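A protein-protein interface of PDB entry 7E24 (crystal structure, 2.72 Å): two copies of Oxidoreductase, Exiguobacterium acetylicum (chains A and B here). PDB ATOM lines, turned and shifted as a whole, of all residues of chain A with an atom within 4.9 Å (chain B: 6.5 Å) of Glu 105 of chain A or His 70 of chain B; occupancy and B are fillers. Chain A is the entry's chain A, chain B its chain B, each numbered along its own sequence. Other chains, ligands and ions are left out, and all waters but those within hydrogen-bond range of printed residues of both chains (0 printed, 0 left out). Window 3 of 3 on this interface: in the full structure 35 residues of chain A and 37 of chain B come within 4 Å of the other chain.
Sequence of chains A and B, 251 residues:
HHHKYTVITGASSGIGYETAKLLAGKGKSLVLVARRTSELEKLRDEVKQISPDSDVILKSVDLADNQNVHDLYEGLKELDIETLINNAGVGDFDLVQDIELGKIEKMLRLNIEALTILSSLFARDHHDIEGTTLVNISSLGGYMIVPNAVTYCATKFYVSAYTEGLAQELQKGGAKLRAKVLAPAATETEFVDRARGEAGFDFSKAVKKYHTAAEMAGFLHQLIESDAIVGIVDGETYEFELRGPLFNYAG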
ATOM      1  N   LEU A 101     -14.660   9.544  33.502  1.00  0.00           N
ATOM      2  CA  LEU A 101     -13.838  10.021  32.398  1.00  0.00           C
ATOM      3  C   LEU A 101     -14.687  10.403  31.193  1.00  0.00           C
ATOM      4  O   LEU A 101     -14.343  11.341  30.461  1.00  0.00           O
ATOM      5  CB  LEU A 101     -12.805   8.971  32.013  1.00  0.00           C
ATOM      6  CG  LEU A 101     -11.670   8.784  33.021  1.00  0.00           C
ATOM      7  CD1 LEU A 101     -11.887   7.508  33.822  1.00  0.00           C
ATOM      8  CD2 LEU A 101     -10.346   8.788  32.296  1.00  0.00           C
ATOM      9  N   GLY A 102     -15.785   9.681  30.947  1.00  0.00           N
ATOM     10  CA  GLY A 102     -16.619  10.033  29.812  1.00  0.00           C
ATOM     11  C   GLY A 102     -17.128  11.454  29.904  1.00  0.00           C
ATOM     12  O   GLY A 102     -17.095  12.211  28.927  1.00  0.00           O
ATOM     13  N   LYS A 103     -17.547  11.854  31.103  1.00  0.00           N
ATOM     14  CA  LYS A 103     -18.017  13.217  31.298  1.00  0.00           C
ATOM     15  C   LYS A 103     -16.861  14.199  31.203  1.00  0.00           C
ATOM     16  O   LYS A 103     -16.976  15.245  30.559  1.00  0.00           O
ATOM     17  CB  LYS A 103     -18.713  13.347  32.646  1.00  0.00           C
ATOM     18  CG  LYS A 103     -19.360  14.687  32.838  1.00  0.00           C
ATOM     19  CD  LYS A 103     -19.745  14.927  34.286  1.00  0.00           C
ATOM     20  CE  LYS A 103     -20.206  16.375  34.485  1.00  0.00           C
ATOM     21  NZ  LYS A 103     -20.292  16.836  35.896  1.00  0.00           N
ATOM     22  N   ILE A 104     -15.727  13.865  31.826  1.00  0.00           N
ATOM     23  CA  ILE A 104     -14.585  14.773  31.851  1.00  0.00           C
ATOM     24  C   ILE A 104     -14.001  14.927  30.451  1.00  0.00           C
ATOM     25  O   ILE A 104     -13.689  16.045  30.017  1.00  0.00           O
ATOM     26  CB  ILE A 104     -13.531  14.288  32.865  1.00  0.00           C
ATOM     27  CG1 ILE A 104     -13.690  15.026  34.186  1.00  0.00           C
ATOM     28  CG2 ILE A 104     -12.136  14.542  32.347  1.00  0.00           C
ATOM     29  CD1 ILE A 104     -15.064  14.894  34.776  1.00  0.00           C
ATOM     30  N   GLU A 105     -13.866  13.811  29.717  1.00  0.00           N
ATOM     31  CA  GLU A 105     -13.426  13.880  28.329  1.00  0.00           C
ATOM     32  C   GLU A 105     -14.341  14.789  27.531  1.00  0.00           C
ATOM     33  O   GLU A 105     -13.868  15.641  26.773  1.00  0.00           O
ATOM     34  CB  GLU A 105     -13.378  12.482  27.713  1.00  0.00           C
ATOM     35  CG  GLU A 105     -12.129  11.696  28.080  1.00  0.00           C
ATOM     36  CD  GLU A 105     -12.274  10.210  27.822  1.00  0.00           C
ATOM     37  OE1 GLU A 105     -13.080   9.846  26.934  1.00  0.00           O
ATOM     38  OE2 GLU A 105     -11.578   9.409  28.496  1.00  0.00           O
ATOM     39  N   LYS A 106     -15.656  14.649  27.718  1.00  0.00           N
ATOM     40  CA  LYS A 106     -16.595  15.532  27.036  1.00  0.00           C
ATOM     41  C   LYS A 106     -16.375  16.973  27.465  1.00  0.00           C
ATOM     42  O   LYS A 106     -16.361  17.880  26.627  1.00  0.00           O
ATOM     43  CB  LYS A 106     -18.021  15.077  27.315  1.00  0.00           C
ATOM     44  CG  LYS A 106     -19.062  15.524  26.326  1.00  0.00           C
ATOM     45  CD  LYS A 106     -20.451  15.346  26.931  1.00  0.00           C
ATOM     46  CE  LYS A 106     -21.558  15.478  25.885  1.00  0.00           C
ATOM     47  NZ  LYS A 106     -22.940  15.425  26.444  1.00  0.00           N
ATOM     48  N   MET A 107     -16.147  17.198  28.760  1.00  0.00           N
ATOM     49  CA  MET A 107     -15.830  18.546  29.224  1.00  0.00           C
ATOM     50  C   MET A 107     -14.638  19.134  28.474  1.00  0.00           C
ATOM     51  O   MET A 107     -14.675  20.291  28.039  1.00  0.00           O
ATOM     52  CB  MET A 107     -15.559  18.546  30.721  1.00  0.00           C
ATOM     53  CG  MET A 107     -15.283  19.921  31.245  1.00  0.00           C
ATOM     54  SD  MET A 107     -15.008  19.967  33.021  1.00  0.00           S
ATOM     55  CE  MET A 107     -13.624  18.849  33.249  1.00  0.00           C
ATOM     56  N   LEU A 108     -13.572  18.352  28.295  1.00  0.00           N
ATOM     57  CA  LEU A 108     -12.417  18.878  27.574  1.00  0.00           C
ATOM     58  C   LEU A 108     -12.786  19.227  26.135  1.00  0.00           C
ATOM     59  O   LEU A 108     -12.343  20.248  25.600  1.00  0.00           O
ATOM     60  CB  LEU A 108     -11.271  17.875  27.591  1.00  0.00           C
ATOM     61  CG  LEU A 108     -10.737  17.457  28.966  1.00  0.00           C
ATOM     62  CD1 LEU A 108      -9.650  16.456  28.789  1.00  0.00           C
ATOM     63  CD2 LEU A 108     -10.225  18.643  29.719  1.00  0.00           C
ATOM     64  N   ARG A 109     -13.600  18.388  25.486  1.00  0.00           N
ATOM     65  CA  ARG A 109     -13.933  18.639  24.085  1.00  0.00           C
ATOM     66  C   ARG A 109     -14.773  19.896  23.934  1.00  0.00           C
ATOM     67  O   ARG A 109     -14.672  20.589  22.910  1.00  0.00           O
ATOM     68  CB  ARG A 109     -14.683  17.452  23.493  1.00  0.00           C
ATOM     69  CG  ARG A 109     -13.978  16.145  23.612  1.00  0.00           C
ATOM     70  CD  ARG A 109     -14.606  15.123  22.673  1.00  0.00           C
ATOM     71  NE  ARG A 109     -15.785  14.485  23.244  1.00  0.00           N
ATOM     72  CZ  ARG A 109     -15.734  13.413  24.031  1.00  0.00           C
ATOM     73  NH1 ARG A 109     -14.558  12.866  24.341  1.00  0.00           N
ATOM     74  NH2 ARG A 109     -16.851  12.891  24.524  1.00  0.00           N
ATOM     75  N   ASP B  65      -5.369   9.527  20.194  1.00  0.00           N
ATOM     76  CA  ASP B  65      -6.704   8.953  20.152  1.00  0.00           C
ATOM     77  C   ASP B  65      -7.109   8.565  21.567  1.00  0.00           C
ATOM     78  O   ASP B  65      -6.378   7.824  22.237  1.00  0.00           O
ATOM     79  CB  ASP B  65      -6.735   7.723  19.246  1.00  0.00           C
ATOM     80  CG  ASP B  65      -8.119   7.106  19.140  1.00  0.00           C
ATOM     81  OD1 ASP B  65      -8.537   6.406  20.069  1.00  0.00           O
ATOM     82  OD2 ASP B  65      -8.800   7.346  18.130  1.00  0.00           O
ATOM     83  N   ASN B  66      -8.276   9.047  22.020  1.00  0.00           N
ATOM     84  CA  ASN B  66      -8.667   8.815  23.412  1.00  0.00           C
ATOM     85  C   ASN B  66      -8.878   7.331  23.691  1.00  0.00           C
ATOM     86  O   ASN B  66      -8.465   6.823  24.744  1.00  0.00           O
ATOM     87  CB  ASN B  66      -9.924   9.608  23.754  1.00  0.00           C
ATOM     88  CG  ASN B  66      -9.660  11.087  23.834  1.00  0.00           C
ATOM     89  OD1 ASN B  66      -8.502  11.502  23.821  1.00  0.00           O
ATOM     90  ND2 ASN B  66     -10.710  11.896  23.889  1.00  0.00           N
ATOM     91  N   GLN B  67      -9.500   6.611  22.751  1.00  0.00           N
ATOM     92  CA  GLN B  67      -9.705   5.186  22.960  1.00  0.00           C
ATOM     93  C   GLN B  67      -8.369   4.472  23.107  1.00  0.00           C
ATOM     94  O   GLN B  67      -8.203   3.630  23.997  1.00  0.00           O
ATOM     95  CB  GLN B  67     -10.537   4.614  21.817  1.00  0.00           C
ATOM     96  CG  GLN B  67     -10.883   3.144  21.962  1.00  0.00           C
ATOM     97  CD  GLN B  67     -11.459   2.804  23.324  1.00  0.00           C
ATOM     98  OE1 GLN B  67     -12.378   3.473  23.805  1.00  0.00           O
ATOM     99  NE2 GLN B  67     -10.930   1.752  23.949  1.00  0.00           N
ATOM    100  N   ASN B  68      -7.382   4.843  22.284  1.00  0.00           N
ATOM    101  CA  ASN B  68      -6.069   4.214  22.375  1.00  0.00           C
ATOM    102  C   ASN B  68      -5.476   4.377  23.763  1.00  0.00           C
ATOM    103  O   ASN B  68      -4.835   3.457  24.280  1.00  0.00           O
ATOM    104  CB  ASN B  68      -5.114   4.819  21.352  1.00  0.00           C
ATOM    105  CG  ASN B  68      -5.282   4.245  19.985  1.00  0.00           C
ATOM    106  OD1 ASN B  68      -6.105   3.360  19.766  1.00  0.00           O
ATOM    107  ND2 ASN B  68      -4.491   4.737  19.050  1.00  0.00           N
ATOM    108  N   VAL B  69      -5.678   5.543  24.382  1.00  0.00           N
ATOM    109  CA  VAL B  69      -5.090   5.807  25.692  1.00  0.00           C
ATOM    110  C   VAL B  69      -5.721   4.911  26.752  1.00  0.00           C
ATOM    111  O   VAL B  69      -5.021   4.319  27.576  1.00  0.00           O
ATOM    112  CB  VAL B  69      -5.222   7.298  26.038  1.00  0.00           C
ATOM    113  CG1 VAL B  69      -4.630   7.586  27.425  1.00  0.00           C
ATOM    114  CG2 VAL B  69      -4.517   8.122  24.991  1.00  0.00           C
ATOM    115  N   HIS B  70      -7.048   4.772  26.722  1.00  0.00           N
ATOM    116  CA  HIS B  70      -7.720   3.812  27.587  1.00  0.00           C
ATOM    117  C   HIS B  70      -7.184   2.403  27.366  1.00  0.00           C
ATOM    118  O   HIS B  70      -6.885   1.685  28.325  1.00  0.00           O
ATOM    119  CB  HIS B  70      -9.218   3.858  27.322  1.00  0.00           C
ATOM    120  CG  HIS B  70      -9.917   5.027  27.944  1.00  0.00           C
ATOM    121  ND1 HIS B  70     -10.348   5.032  29.254  1.00  0.00           N
ATOM    122  CD2 HIS B  70     -10.266   6.230  27.432  1.00  0.00           C
ATOM    123  CE1 HIS B  70     -10.939   6.183  29.519  1.00  0.00           C
ATOM    124  NE2 HIS B  70     -10.899   6.930  28.431  1.00  0.00           N
ATOM    125  N   ASP B  71      -7.041   1.996  26.100  1.00  0.00           N
ATOM    126  CA  ASP B  71      -6.570   0.648  25.791  1.00  0.00           C
ATOM    127  C   ASP B  71      -5.156   0.431  26.309  1.00  0.00           C
ATOM    128  O   ASP B  71      -4.834  -0.631  26.853  1.00  0.00           O
ATOM    129  CB  ASP B  71      -6.619   0.416  24.287  1.00  0.00           C
ATOM    130  CG  ASP B  71      -8.025   0.362  23.758  1.00  0.00           C
ATOM    131  OD1 ASP B  71      -8.958   0.455  24.585  1.00  0.00           O
ATOM    132  OD2 ASP B  71      -8.194   0.271  22.521  1.00  0.00           O
ATOM    133  N   LEU B  72      -4.293   1.433  26.143  1.00  0.00           N
ATOM    134  CA  LEU B  72      -2.951   1.351  26.700  1.00  0.00           C
ATOM    135  C   LEU B  72      -3.003   1.050  28.191  1.00  0.00           C
ATOM    136  O   LEU B  72      -2.252   0.209  28.686  1.00  0.00           O
ATOM    137  CB  LEU B  72      -2.205   2.649  26.454  1.00  0.00           C
ATOM    138  CG  LEU B  72      -1.007   2.801  27.376  1.00  0.00           C
ATOM    139  CD1 LEU B  72       0.116   1.881  26.939  1.00  0.00           C
ATOM    140  CD2 LEU B  72      -0.576   4.252  27.442  1.00  0.00           C
ATOM    141  N   TYR B  73      -3.914   1.703  28.922  1.00  0.00           N
ATOM    142  CA  TYR B  73      -3.901   1.601  30.377  1.00  0.00           C
ATOM    143  C   TYR B  73      -4.510   0.291  30.843  1.00  0.00           C
ATOM    144  O   TYR B  73      -3.936  -0.403  31.682  1.00  0.00           O
ATOM    145  CB  TYR B  73      -4.650   2.771  31.003  1.00  0.00           C
ATOM    146  CG  TYR B  73      -4.525   2.786  32.515  1.00  0.00           C
ATOM    147  CD1 TYR B  73      -3.441   3.390  33.135  1.00  0.00           C
ATOM    148  CD2 TYR B  73      -5.490   2.185  33.318  1.00  0.00           C
ATOM    149  CE1 TYR B  73      -3.317   3.402  34.502  1.00  0.00           C
ATOM    150  CE2 TYR B  73      -5.375   2.189  34.694  1.00  0.00           C
ATOM    151  CZ  TYR B  73      -4.276   2.798  35.275  1.00  0.00           C
ATOM    152  OH  TYR B  73      -4.104   2.828  36.636  1.00  0.00           O
ATOM    153  N   GLU B  74      -5.701  -0.032  30.343  1.00  0.00           N
ATOM    154  CA  GLU B  74      -6.356  -1.298  30.652  1.00  0.00           C
ATOM    155  C   GLU B  74      -5.449  -2.494  30.366  1.00  0.00           C
ATOM    156  O   GLU B  74      -5.502  -3.508  31.066  1.00  0.00           O
ATOM    157  CB  GLU B  74      -7.646  -1.362  29.846  1.00  0.00           C
ATOM    158  CG  GLU B  74      -8.247  -2.729  29.664  1.00  0.00           C
ATOM    159  CD  GLU B  74      -8.730  -3.332  30.953  1.00  0.00           C
ATOM    160  OE1 GLU B  74      -8.903  -2.589  31.949  1.00  0.00           O
ATOM    161  OE2 GLU B  74      -8.979  -4.557  30.950  1.00  0.00           O
ATOM    162  N   GLY B  75      -4.593  -2.392  29.354  1.00  0.00           N
ATOM    163  CA  GLY B  75      -3.652  -3.466  29.084  1.00  0.00           C
ATOM    164  C   GLY B  75      -2.504  -3.555  30.058  1.00  0.00           C
ATOM    165  O   GLY B  75      -1.775  -4.552  30.032  1.00  0.00           O
ATOM    166  N   GLU B 113      -5.485  15.710  26.606  1.00  0.00           N
ATOM    167  CA  GLU B 113      -6.420  14.631  26.912  1.00  0.00           C
ATOM    168  C   GLU B 113      -5.722  13.358  27.350  1.00  0.00           C
ATOM    169  O   GLU B 113      -6.089  12.762  28.368  1.00  0.00           O
ATOM    170  CB  GLU B 113      -7.272  14.356  25.697  1.00  0.00           C
ATOM    171  CG  GLU B 113      -8.214  15.453  25.450  1.00  0.00           C
ATOM    172  CD  GLU B 113      -9.102  15.175  24.315  1.00  0.00           C
ATOM    173  OE1 GLU B 113      -9.031  14.064  23.768  1.00  0.00           O
ATOM    174  OE2 GLU B 113      -9.915  16.044  23.983  1.00  0.00           O
ATOM    175  N   ILE B 117      -6.360  11.602  30.809  1.00  0.00           N
ATOM    176  CA  ILE B 117      -6.881  10.247  30.961  1.00  0.00           C
ATOM    177  C   ILE B 117      -5.928   9.408  31.805  1.00  0.00           C
ATOM    178  O   ILE B 117      -6.333   8.765  32.775  1.00  0.00           O
ATOM    179  CB  ILE B 117      -7.116   9.603  29.583  1.00  0.00           C
ATOM    180  CG1 ILE B 117      -8.284  10.264  28.852  1.00  0.00           C
ATOM    181  CG2 ILE B 117      -7.384   8.123  29.731  1.00  0.00           C
ATOM    182  CD1 ILE B 117      -8.128  10.217  27.376  1.00  0.00           C
ATOM    183  N   LEU B 118      -4.637   9.424  31.463  1.00  0.00           N
ATOM    184  CA  LEU B 118      -3.687   8.561  32.157  1.00  0.00           C
ATOM    185  C   LEU B 118      -3.525   8.983  33.611  1.00  0.00           C
ATOM    186  O   LEU B 118      -3.418   8.129  34.503  1.00  0.00           O
ATOM    187  CB  LEU B 118      -2.342   8.563  31.432  1.00  0.00           C
ATOM    188  CG  LEU B 118      -2.314   7.826  30.093  1.00  0.00           C
ATOM    189  CD1 LEU B 118      -0.966   7.892  29.434  1.00  0.00           C
ATOM    190  CD2 LEU B 118      -2.754   6.391  30.286  1.00  0.00           C
ATOM    191  N   LEU B 121      -6.774   7.939  35.560  1.00  0.00           N
ATOM    192  CA  LEU B 121      -6.874   6.503  35.766  1.00  0.00           C
ATOM    193  C   LEU B 121      -5.805   6.032  36.735  1.00  0.00           C
ATOM    194  O   LEU B 121      -6.082   5.226  37.632  1.00  0.00           O
ATOM    195  CB  LEU B 121      -6.768   5.771  34.428  1.00  0.00           C
ATOM    196  CG  LEU B 121      -7.918   5.893  33.423  1.00  0.00           C
ATOM    197  CD1 LEU B 121      -7.469   5.331  32.112  1.00  0.00           C
ATOM    198  CD2 LEU B 121      -9.154   5.176  33.901  1.00  0.00           C
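The side-chain carboxylate of Glu 105 of chain A lies within hydrogen-bond range of a ring nitrogen (NE2) of His 70 of chain B (2.6 Å).
The side-chain carboxylate of Glu 113 of chain B sits close to the side-chain amide oxygen of Asn 66 of chain B (2.6 Å). The backbone carbonyl oxygen (O) of Leu 121 of chain B lies within hydrogen-bond range of the side-chain hydroxyl (OH) of Tyr 73 of chain B.
Leu 101 of chain A touches His 70 of chain B (CD2 to CE1, 3.9 Å). Ile 117 of chain B touches Leu 101 of chain A (CG2 to CD2, 3.97 Å). Leu 121 of chain B touches Leu 101 of chain A (CD2 to CD1, 3.6 Å). OE2 of Glu 105 of chain A touches CG1 of Ile 117 of chain B, 3.4 Å away. CD1 of Leu 108 of chain A touches CG of Glu 113 of chain B (3.8 Å). Arg 109 of chain A touches Asn 66 of chain B (NH1 to ND2, 3.99 Å).
Glu 105 of chain A touches two residues of chain B. His 70 of chain B touches just these residues of chain A: Leu 101 and Glu 105. Of the printed residues of chain A, Asn 66 of chain B touches Arg 109 (3.99 Å). Of the printed residues of chain B, Leu 108 of chain A touches Glu 113 (3.8 Å). Of the printed residues of chain B, Leu 101 of chain A touches His 70 (3.9 Å), Ile 117 (3.97 Å) and Leu 121 (3.6 Å). Printed residues of chain A within 4 Å of Ile 117 of chain B: Leu 101 and Glu 105. Asn 68 of chain B touches none of the printed residues of chain A. Asp 65 of chain B touches none of the printed residues of chain A. The nearest residue of chain B that does not touch Glu 105 of chain A is Asn 66 of chain B (4.4 Å). The nearest printed residue of chain A that does not touch His 70 of chain B is Gly 102 of chain A (6.1 Å). The nearest printed residue of chain B that does not touch Arg 109 of chain A is Glu 113 of chain B (4.1 Å).
Printed residues of chain A that touch a printed residue of chain B: Leu 101, Glu 105, Leu 108 and Arg 109. Hydrophobic or aromatic side chains of chain A within 4 Å of the printed part of chain B: Leu 101 and Leu 108. Of the 15 printed residues of chain B, 5 touch a printed residue of chain A. Hydrophobic or aromatic side chains of chain B within 4 Å of the printed part of chain A: His 70, Ile 117 and Leu 121.
No position is printed for both chains. Of the 7 pairs that touch across the chains among the printed residues, none has its exchanged pair printed and touching as well.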
